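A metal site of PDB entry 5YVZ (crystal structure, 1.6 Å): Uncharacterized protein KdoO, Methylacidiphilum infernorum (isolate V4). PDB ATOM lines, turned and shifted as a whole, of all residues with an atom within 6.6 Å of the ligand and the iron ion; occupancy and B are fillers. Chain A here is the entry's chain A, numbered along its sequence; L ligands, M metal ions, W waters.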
ATOM      1  N   ARG A 127     -32.859  12.167  29.993  1.00  0.00           N
ATOM      2  CA  ARG A 127     -32.921  10.845  30.625  1.00  0.00           C
ATOM      3  C   ARG A 127     -32.464  10.972  32.077  1.00  0.00           C
ATOM      4  O   ARG A 127     -31.249  10.882  32.366  1.00  0.00           O
ATOM      5  CB  ARG A 127     -32.074   9.847  29.854  1.00  0.00           C
ATOM      6  CG  ARG A 127     -32.339   9.896  28.357  1.00  0.00           C
ATOM      7  CD  ARG A 127     -31.692   8.730  27.630  1.00  0.00           C
ATOM      8  NE  ARG A 127     -31.905   8.849  26.190  1.00  0.00           N
ATOM      9  CZ  ARG A 127     -31.173   8.234  25.279  1.00  0.00           C
ATOM     10  NH1 ARG A 127     -30.164   7.466  25.664  1.00  0.00           N
ATOM     11  NH2 ARG A 127     -31.427   8.383  23.985  1.00  0.00           N
ATOM     12  N   ILE A 131     -29.230   4.317  35.329  1.00  0.00           N
ATOM     13  CA  ILE A 131     -29.184   3.170  34.418  1.00  0.00           C
ATOM     14  C   ILE A 131     -29.014   1.868  35.198  1.00  0.00           C
ATOM     15  O   ILE A 131     -29.648   0.862  34.873  1.00  0.00           O
ATOM     16  CB  ILE A 131     -28.046   3.348  33.387  1.00  0.00           C
ATOM     17  CG1 ILE A 131     -28.394   4.438  32.381  1.00  0.00           C
ATOM     18  CG2 ILE A 131     -27.746   2.022  32.686  1.00  0.00           C
ATOM     19  CD1 ILE A 131     -29.506   4.057  31.438  1.00  0.00           C
ATOM     20  N   ASP A 142     -30.731  -1.989  27.119  1.00  0.00           N
ATOM     21  CA  ASP A 142     -29.639  -1.281  26.480  1.00  0.00           C
ATOM     22  C   ASP A 142     -28.303  -1.479  27.187  1.00  0.00           C
ATOM     23  O   ASP A 142     -27.318  -0.840  26.803  1.00  0.00           O
ATOM     24  CB  ASP A 142     -29.980   0.209  26.346  1.00  0.00           C
ATOM     25  CG  ASP A 142     -30.791   0.484  25.090  1.00  0.00           C
ATOM     26  OD1 ASP A 142     -31.193  -0.493  24.415  1.00  0.00           O
ATOM     27  OD2 ASP A 142     -31.032   1.673  24.768  1.00  0.00           O
ATOM     28  N   HIS A 146     -25.685  -3.209  20.887  1.00  0.00           N
ATOM     29  CA  HIS A 146     -26.626  -3.106  19.783  1.00  0.00           C
ATOM     30  C   HIS A 146     -26.259  -1.912  18.913  1.00  0.00           C
ATOM     31  O   HIS A 146     -25.531  -1.014  19.346  1.00  0.00           O
ATOM     32  CB  HIS A 146     -28.053  -2.928  20.290  1.00  0.00           C
ATOM     33  CG  HIS A 146     -28.245  -1.633  21.016  1.00  0.00           C
ATOM     34  ND1 HIS A 146     -27.786  -1.435  22.306  1.00  0.00           N
ATOM     35  CD2 HIS A 146     -28.752  -0.448  20.606  1.00  0.00           C
ATOM     36  CE1 HIS A 146     -28.044  -0.183  22.668  1.00  0.00           C
ATOM     37  NE2 HIS A 146     -28.637   0.432  21.651  1.00  0.00           N
ATOM     38  N   VAL A 147     -26.784  -1.915  17.691  1.00  0.00           N
ATOM     39  CA  VAL A 147     -26.953  -0.695  16.923  1.00  0.00           C
ATOM     40  C   VAL A 147     -28.415  -0.290  17.046  1.00  0.00           C
ATOM     41  O   VAL A 147     -29.290  -1.112  17.331  1.00  0.00           O
ATOM     42  CB  VAL A 147     -26.529  -0.849  15.445  1.00  0.00           C
ATOM     43  CG1 VAL A 147     -25.037  -1.179  15.348  1.00  0.00           C
ATOM     44  CG2 VAL A 147     -27.372  -1.916  14.738  1.00  0.00           C
ATOM     45  N   ASP A 148     -28.667   1.001  16.861  1.00  0.00           N
ATOM     46  CA  ASP A 148     -30.012   1.531  17.065  1.00  0.00           C
ATOM     47  C   ASP A 148     -30.922   1.149  15.911  1.00  0.00           C
ATOM     48  O   ASP A 148     -30.585   1.348  14.737  1.00  0.00           O
ATOM     49  CB  ASP A 148     -29.973   3.046  17.218  1.00  0.00           C
ATOM     50  CG  ASP A 148     -29.555   3.481  18.602  1.00  0.00           C
ATOM     51  OD1 ASP A 148     -29.335   2.606  19.476  1.00  0.00           O
ATOM     52  OD2 ASP A 148     -29.448   4.702  18.827  1.00  0.00           O
ATOM     53  N   ALA A 149     -32.074   0.610  16.269  1.00  0.00           N
ATOM     54  CA  ALA A 149     -33.131   0.285  15.327  1.00  0.00           C
ATOM     55  C   ALA A 149     -34.406   0.262  16.139  1.00  0.00           C
ATOM     56  O   ALA A 149     -34.474  -0.420  17.162  1.00  0.00           O
ATOM     57  CB  ALA A 149     -32.894  -1.060  14.633  1.00  0.00           C
ATOM     58  N   PHE A 150     -35.413   1.014  15.711  1.00  0.00           N
ATOM     59  CA  PHE A 150     -36.613   1.178  16.507  1.00  0.00           C
ATOM     60  C   PHE A 150     -37.804   0.609  15.764  1.00  0.00           C
ATOM     61  O   PHE A 150     -38.108   1.052  14.649  1.00  0.00           O
ATOM     62  CB  PHE A 150     -36.812   2.655  16.838  1.00  0.00           C
ATOM     63  CG  PHE A 150     -35.631   3.264  17.510  1.00  0.00           C
ATOM     64  CD1 PHE A 150     -35.328   2.953  18.827  1.00  0.00           C
ATOM     65  CD2 PHE A 150     -34.768   4.105  16.818  1.00  0.00           C
ATOM     66  CE1 PHE A 150     -34.223   3.495  19.453  1.00  0.00           C
ATOM     67  CE2 PHE A 150     -33.651   4.645  17.438  1.00  0.00           C
ATOM     68  CZ  PHE A 150     -33.385   4.340  18.758  1.00  0.00           C
ATOM     69  N   ARG A 162     -26.324  10.737  16.823  1.00  0.00           N
ATOM     70  CA  ARG A 162     -26.713  11.237  18.142  1.00  0.00           C
ATOM     71  C   ARG A 162     -25.581  12.007  18.790  1.00  0.00           C
ATOM     72  O   ARG A 162     -24.407  11.630  18.712  1.00  0.00           O
ATOM     73  CB  ARG A 162     -27.158  10.083  19.054  1.00  0.00           C
ATOM     74  CG  ARG A 162     -28.447   9.464  18.512  1.00  0.00           C
ATOM     75  CD  ARG A 162     -29.087   8.457  19.461  1.00  0.00           C
ATOM     76  NE  ARG A 162     -30.534   8.464  19.256  1.00  0.00           N
ATOM     77  CZ  ARG A 162     -31.389   7.666  19.879  1.00  0.00           C
ATOM     78  NH1 ARG A 162     -30.961   6.773  20.756  1.00  0.00           N
ATOM     79  NH2 ARG A 162     -32.691   7.785  19.630  1.00  0.00           N
ATOM     80  N   PHE A 164     -24.568  13.313  22.627  1.00  0.00           N
ATOM     81  CA  PHE A 164     -24.846  12.995  24.026  1.00  0.00           C
ATOM     82  C   PHE A 164     -24.076  13.937  24.928  1.00  0.00           C
ATOM     83  O   PHE A 164     -22.924  14.257  24.656  1.00  0.00           O
ATOM     84  CB  PHE A 164     -24.372  11.573  24.369  1.00  0.00           C
ATOM     85  CG  PHE A 164     -25.078  10.485  23.642  1.00  0.00           C
ATOM     86  CD1 PHE A 164     -26.221   9.901  24.179  1.00  0.00           C
ATOM     87  CD2 PHE A 164     -24.570   9.988  22.451  1.00  0.00           C
ATOM     88  CE1 PHE A 164     -26.865   8.852  23.510  1.00  0.00           C
ATOM     89  CE2 PHE A 164     -25.207   8.932  21.783  1.00  0.00           C
ATOM     90  CZ  PHE A 164     -26.357   8.385  22.327  1.00  0.00           C
ATOM     91  N   ARG A 174     -20.804   8.343  32.872  1.00  0.00           N
ATOM     92  CA  ARG A 174     -21.748   7.462  32.194  1.00  0.00           C
ATOM     93  C   ARG A 174     -20.937   6.341  31.558  1.00  0.00           C
ATOM     94  O   ARG A 174     -20.080   6.594  30.695  1.00  0.00           O
ATOM     95  CB  ARG A 174     -22.567   8.203  31.154  1.00  0.00           C
ATOM     96  CG  ARG A 174     -23.826   7.431  30.768  1.00  0.00           C
ATOM     97  CD  ARG A 174     -24.840   8.331  30.186  1.00  0.00           C
ATOM     98  NE  ARG A 174     -26.122   7.662  29.943  1.00  0.00           N
ATOM     99  CZ  ARG A 174     -27.171   7.724  30.762  1.00  0.00           C
ATOM    100  NH1 ARG A 174     -27.084   8.400  31.898  1.00  0.00           N
ATOM    101  NH2 ARG A 174     -28.298   7.116  30.424  1.00  0.00           N
ATOM    102  N   SER A 175     -21.221   5.117  31.974  1.00  0.00           N
ATOM    103  CA  SER A 175     -20.402   3.948  31.637  1.00  0.00           C
ATOM    104  C   SER A 175     -20.969   3.292  30.395  1.00  0.00           C
ATOM    105  O   SER A 175     -22.081   2.748  30.423  1.00  0.00           O
ATOM    106  CB  SER A 175     -20.362   2.962  32.794  1.00  0.00           C
ATOM    107  OG  SER A 175     -19.774   3.573  33.923  1.00  0.00           O
ATOM    108  N   TRP A 176     -20.217   3.360  29.302  1.00  0.00           N
ATOM    109  CA  TRP A 176     -20.571   2.704  28.049  1.00  0.00           C
ATOM    110  C   TRP A 176     -19.648   1.532  27.789  1.00  0.00           C
ATOM    111  O   TRP A 176     -18.538   1.432  28.322  1.00  0.00           O
ATOM    112  CB  TRP A 176     -20.448   3.665  26.861  1.00  0.00           C
ATOM    113  CG  TRP A 176     -21.684   4.439  26.528  1.00  0.00           C
ATOM    114  CD1 TRP A 176     -22.648   4.873  27.379  1.00  0.00           C
ATOM    115  CD2 TRP A 176     -22.074   4.875  25.218  1.00  0.00           C
ATOM    116  NE1 TRP A 176     -23.635   5.562  26.682  1.00  0.00           N
ATOM    117  CE2 TRP A 176     -23.293   5.568  25.355  1.00  0.00           C
ATOM    118  CE3 TRP A 176     -21.497   4.739  23.957  1.00  0.00           C
ATOM    119  CZ2 TRP A 176     -23.967   6.123  24.263  1.00  0.00           C
ATOM    120  CZ3 TRP A 176     -22.162   5.288  22.853  1.00  0.00           C
ATOM    121  CH2 TRP A 176     -23.379   5.972  23.032  1.00  0.00           C
ATOM    122  N   HIS A 225     -30.227  -5.886  15.610  1.00  0.00           N
ATOM    123  CA  HIS A 225     -30.465  -5.388  16.954  1.00  0.00           C
ATOM    124  C   HIS A 225     -30.966  -6.499  17.881  1.00  0.00           C
ATOM    125  O   HIS A 225     -30.366  -6.793  18.913  1.00  0.00           O
ATOM    126  CB  HIS A 225     -31.466  -4.230  16.863  1.00  0.00           C
ATOM    127  CG  HIS A 225     -31.895  -3.670  18.179  1.00  0.00           C
ATOM    128  ND1 HIS A 225     -32.860  -4.252  18.958  1.00  0.00           N
ATOM    129  CD2 HIS A 225     -31.523  -2.528  18.818  1.00  0.00           C
ATOM    130  CE1 HIS A 225     -33.051  -3.517  20.049  1.00  0.00           C
ATOM    131  NE2 HIS A 225     -32.258  -2.474  19.980  1.00  0.00           N
ATOM    132  N   TRP A 251     -20.350  13.572  23.595  1.00  0.00           N
ATOM    133  CA  TRP A 251     -19.815  12.691  22.555  1.00  0.00           C
ATOM    134  C   TRP A 251     -20.824  12.553  21.430  1.00  0.00           C
ATOM    135  O   TRP A 251     -22.014  12.824  21.597  1.00  0.00           O
ATOM    136  CB  TRP A 251     -19.393  11.309  23.121  1.00  0.00           C
ATOM    137  CG  TRP A 251     -20.455  10.482  23.833  1.00  0.00           C
ATOM    138  CD1 TRP A 251     -21.067   9.355  23.351  1.00  0.00           C
ATOM    139  CD2 TRP A 251     -20.945  10.670  25.169  1.00  0.00           C
ATOM    140  NE1 TRP A 251     -21.920   8.830  24.293  1.00  0.00           N
ATOM    141  CE2 TRP A 251     -21.870   9.624  25.414  1.00  0.00           C
ATOM    142  CE3 TRP A 251     -20.713  11.621  26.172  1.00  0.00           C
ATOM    143  CZ2 TRP A 251     -22.563   9.511  26.620  1.00  0.00           C
ATOM    144  CZ3 TRP A 251     -21.397  11.502  27.364  1.00  0.00           C
ATOM    145  CH2 TRP A 251     -22.327  10.463  27.580  1.00  0.00           C
ATOM    146  N   THR A 255     -25.231   6.044  15.925  1.00  0.00           N
ATOM    147  CA  THR A 255     -25.611   4.906  16.766  1.00  0.00           C
ATOM    148  C   THR A 255     -26.242   3.760  15.983  1.00  0.00           C
ATOM    149  O   THR A 255     -26.471   2.690  16.558  1.00  0.00           O
ATOM    150  CB  THR A 255     -26.561   5.349  17.876  1.00  0.00           C
ATOM    151  OG1 THR A 255     -27.668   6.059  17.307  1.00  0.00           O
ATOM    152  CG2 THR A 255     -25.834   6.283  18.858  1.00  0.00           C
ATOM    153  N   HIS A 260     -22.978  -0.365  20.777  1.00  0.00           N
ATOM    154  CA  HIS A 260     -22.850   0.310  22.060  1.00  0.00           C
ATOM    155  C   HIS A 260     -23.820  -0.282  23.080  1.00  0.00           C
ATOM    156  O   HIS A 260     -24.790  -0.974  22.737  1.00  0.00           O
ATOM    157  CB  HIS A 260     -23.087   1.819  21.925  1.00  0.00           C
ATOM    158  CG  HIS A 260     -24.440   2.158  21.383  1.00  0.00           C
ATOM    159  ND1 HIS A 260     -24.770   1.999  20.052  1.00  0.00           N
ATOM    160  CD2 HIS A 260     -25.563   2.581  22.002  1.00  0.00           C
ATOM    161  CE1 HIS A 260     -26.038   2.344  19.876  1.00  0.00           C
ATOM    162  NE2 HIS A 260     -26.540   2.689  21.043  1.00  0.00           N
ATOM    163  N   ALA A 261     -23.525  -0.009  24.346  1.00  0.00           N
ATOM    164  CA  ALA A 261     -24.349  -0.430  25.479  1.00  0.00           C
ATOM    165  C   ALA A 261     -24.046   0.532  26.604  1.00  0.00           C
ATOM    166  O   ALA A 261     -22.957   1.118  26.652  1.00  0.00           O
ATOM    167  CB  ALA A 261     -24.038  -1.865  25.917  1.00  0.00           C
ATOM    168  N   VAL A 262     -25.010   0.730  27.500  1.00  0.00           N
ATOM    169  CA  VAL A 262     -24.767   1.566  28.673  1.00  0.00           C
ATOM    170  C   VAL A 262     -24.964   0.720  29.920  1.00  0.00           C
ATOM    171  O   VAL A 262     -25.911  -0.065  30.012  1.00  0.00           O
ATOM    172  CB  VAL A 262     -25.668   2.820  28.689  1.00  0.00           C
ATOM    173  CG1 VAL A 262     -27.142   2.449  28.672  1.00  0.00           C
ATOM    174  CG2 VAL A 262     -25.333   3.710  29.895  1.00  0.00           C
ATOM    175  N   LYS A 264     -24.152   2.119  33.429  1.00  0.00           N
ATOM    176  CA  LYS A 264     -24.316   2.879  34.659  1.00  0.00           C
ATOM    177  C   LYS A 264     -24.352   4.358  34.318  1.00  0.00           C
ATOM    178  O   LYS A 264     -23.733   4.800  33.347  1.00  0.00           O
ATOM    179  CB  LYS A 264     -23.183   2.562  35.667  1.00  0.00           C
ATOM    180  CG  LYS A 264     -23.098   3.457  36.886  1.00  0.00           C
ATOM    181  CD  LYS A 264     -21.811   3.189  37.664  1.00  0.00           C
ATOM    182  CE  LYS A 264     -20.593   3.745  36.936  1.00  0.00           C
ATOM    183  NZ  LYS A 264     -20.787   5.154  36.490  1.00  0.00           N
ATOM    184  N   LEU A 268     -28.705  12.510  31.461  1.00  0.00           N
ATOM    185  CA  LEU A 268     -28.147  12.545  30.117  1.00  0.00           C
ATOM    186  C   LEU A 268     -29.052  13.403  29.269  1.00  0.00           C
ATOM    187  O   LEU A 268     -30.281  13.286  29.351  1.00  0.00           O
ATOM    188  CB  LEU A 268     -28.071  11.134  29.539  1.00  0.00           C
ATOM    189  CG  LEU A 268     -27.587  11.015  28.097  1.00  0.00           C
ATOM    190  CD1 LEU A 268     -26.090  11.233  28.042  1.00  0.00           C
ATOM    191  CD2 LEU A 268     -27.962   9.649  27.523  1.00  0.00           C
ATOM    192  N   GLU A 270     -29.655  14.127  25.142  1.00  0.00           N
ATOM    193  CA  GLU A 270     -29.353  13.474  23.888  1.00  0.00           C
ATOM    194  C   GLU A 270     -30.133  14.164  22.794  1.00  0.00           C
ATOM    195  O   GLU A 270     -31.288  14.545  23.003  1.00  0.00           O
ATOM    196  CB  GLU A 270     -29.693  11.976  23.949  1.00  0.00           C
ATOM    197  CG  GLU A 270     -29.424  11.176  22.688  1.00  0.00           C
ATOM    198  CD  GLU A 270     -30.620  11.196  21.758  1.00  0.00           C
ATOM    199  OE1 GLU A 270     -31.742  11.026  22.257  1.00  0.00           O
ATOM    200  OE2 GLU A 270     -30.401  11.329  20.534  1.00  0.00           O
HETATM  201  C1  LIG L   1     -28.949   5.095  22.967  1.00  0.00           C
HETATM  202  O1  LIG L   1     -28.883   4.778  21.757  1.00  0.00           O
HETATM  203  O2  LIG L   1     -29.286   6.266  23.318  1.00  0.00           O
HETATM  204  C2  LIG L   1     -28.619   4.061  23.986  1.00  0.00           C
HETATM  205  O3  LIG L   1     -28.379   2.918  23.618  1.00  0.00           O
HETATM  206  C3  LIG L   1     -28.560   4.454  25.419  1.00  0.00           C
HETATM  207  C4  LIG L   1     -27.274   5.060  25.868  1.00  0.00           C
HETATM  208  C5  LIG L   1     -27.285   5.822  27.145  1.00  0.00           C
HETATM  209  O4  LIG L   1     -26.211   6.330  27.588  1.00  0.00           O
HETATM  210  O5  LIG L   1     -28.360   5.967  27.770  1.00  0.00           O
HETATM  211 FE    FE M   1     -28.728   2.692  21.457  1.00  0.00          FE
HETATM  212  O   HOH W   1     -30.870   2.256  21.838  1.00  0.00           O
HETATM  213  O   HOH W   2     -30.815   5.248  28.172  1.00  0.00           O
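An oxygen (O2) of the ligand is in salt-bridge range of the guanidinium group (NH1) of Arg 127 (2.8 Å).
The indole nitrogen (NE1) of Trp 176 sits at hydrogen-bond distance from an oxygen (O4) of the ligand.
The guanidinium group (NH1) of Arg 162 is in salt-bridge range of an oxygen (O2) of the ligand (3.1 Å).
The guanidinium group (NE) of Arg 174 lies within salt-bridge range of an oxygen (O4) of the ligand (2.7 Å).
The side-chain carboxylate (OD2) of Asp 148 lies within salt-bridge range of the guanidinium group (NH1) of Arg 162, at 3.2 Å.
The side-chain carboxylate (OE2) of Glu 270 is in salt-bridge range of the guanidinium group (NE) of Arg 162, at 3.1 Å.
OD2 of Asp 148 sits at hydrogen-bond distance from OG1 of Thr 255 (2.7 Å).
O of Trp 251 lies within hydrogen-bond range of N of Phe 164.
The backbone NH (N) of Val 262 sits at hydrogen-bond distance from the backbone carbonyl oxygen (O) of Asp 142.
The side-chain carboxylate (OE1) of Glu 270 lies within salt-bridge range of the guanidinium group (NH2) of Arg 127.
The backbone carbonyl oxygen (O) of Leu 268 sits at hydrogen-bond distance from the backbone NH (N) of Arg 127, 2.9 Å away.
The side-chain carboxylate (OD2) of Asp 142 sits close to an oxygen (O3) of the ligand, 3.1 Å away.
Residues that only touch the ligand: Phe 164 (3.5 Å), Val 262 (3.6 Å) and Leu 268 (3.7 Å).
Hydrophobic or aromatic side chains that line the ligand: His 146, Phe 164, Trp 176, His 260, Val 262 and Leu 268.
Of the 22 residues printed, 11 come within 4 Å of the ligand.
Along chain A the residues within 4 Å of the ligand span positions 127 to 268.
Within 4 Å of the iron ion: His 146, Asp 148 and His 260.
The nearest printed residue that does not touch the iron ion is Asp 142 (4.2 Å).
The iron ion is bound by OD1 of Asp 148 (2.1 Å), O1 of the ligand (2.1 Å), O3 of the ligand (2.2 Å), water W1 (2.2 Å), NE2 of His 260 (2.2 Å) and NE2 of His 146 (2.3 Å).
The iron ion has six donor atoms within binding distance.
Water W2 lies within hydrogen-bond range of O5 of the ligand (2.6 Å) and NH1 of Arg 127 (3.4 Å).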
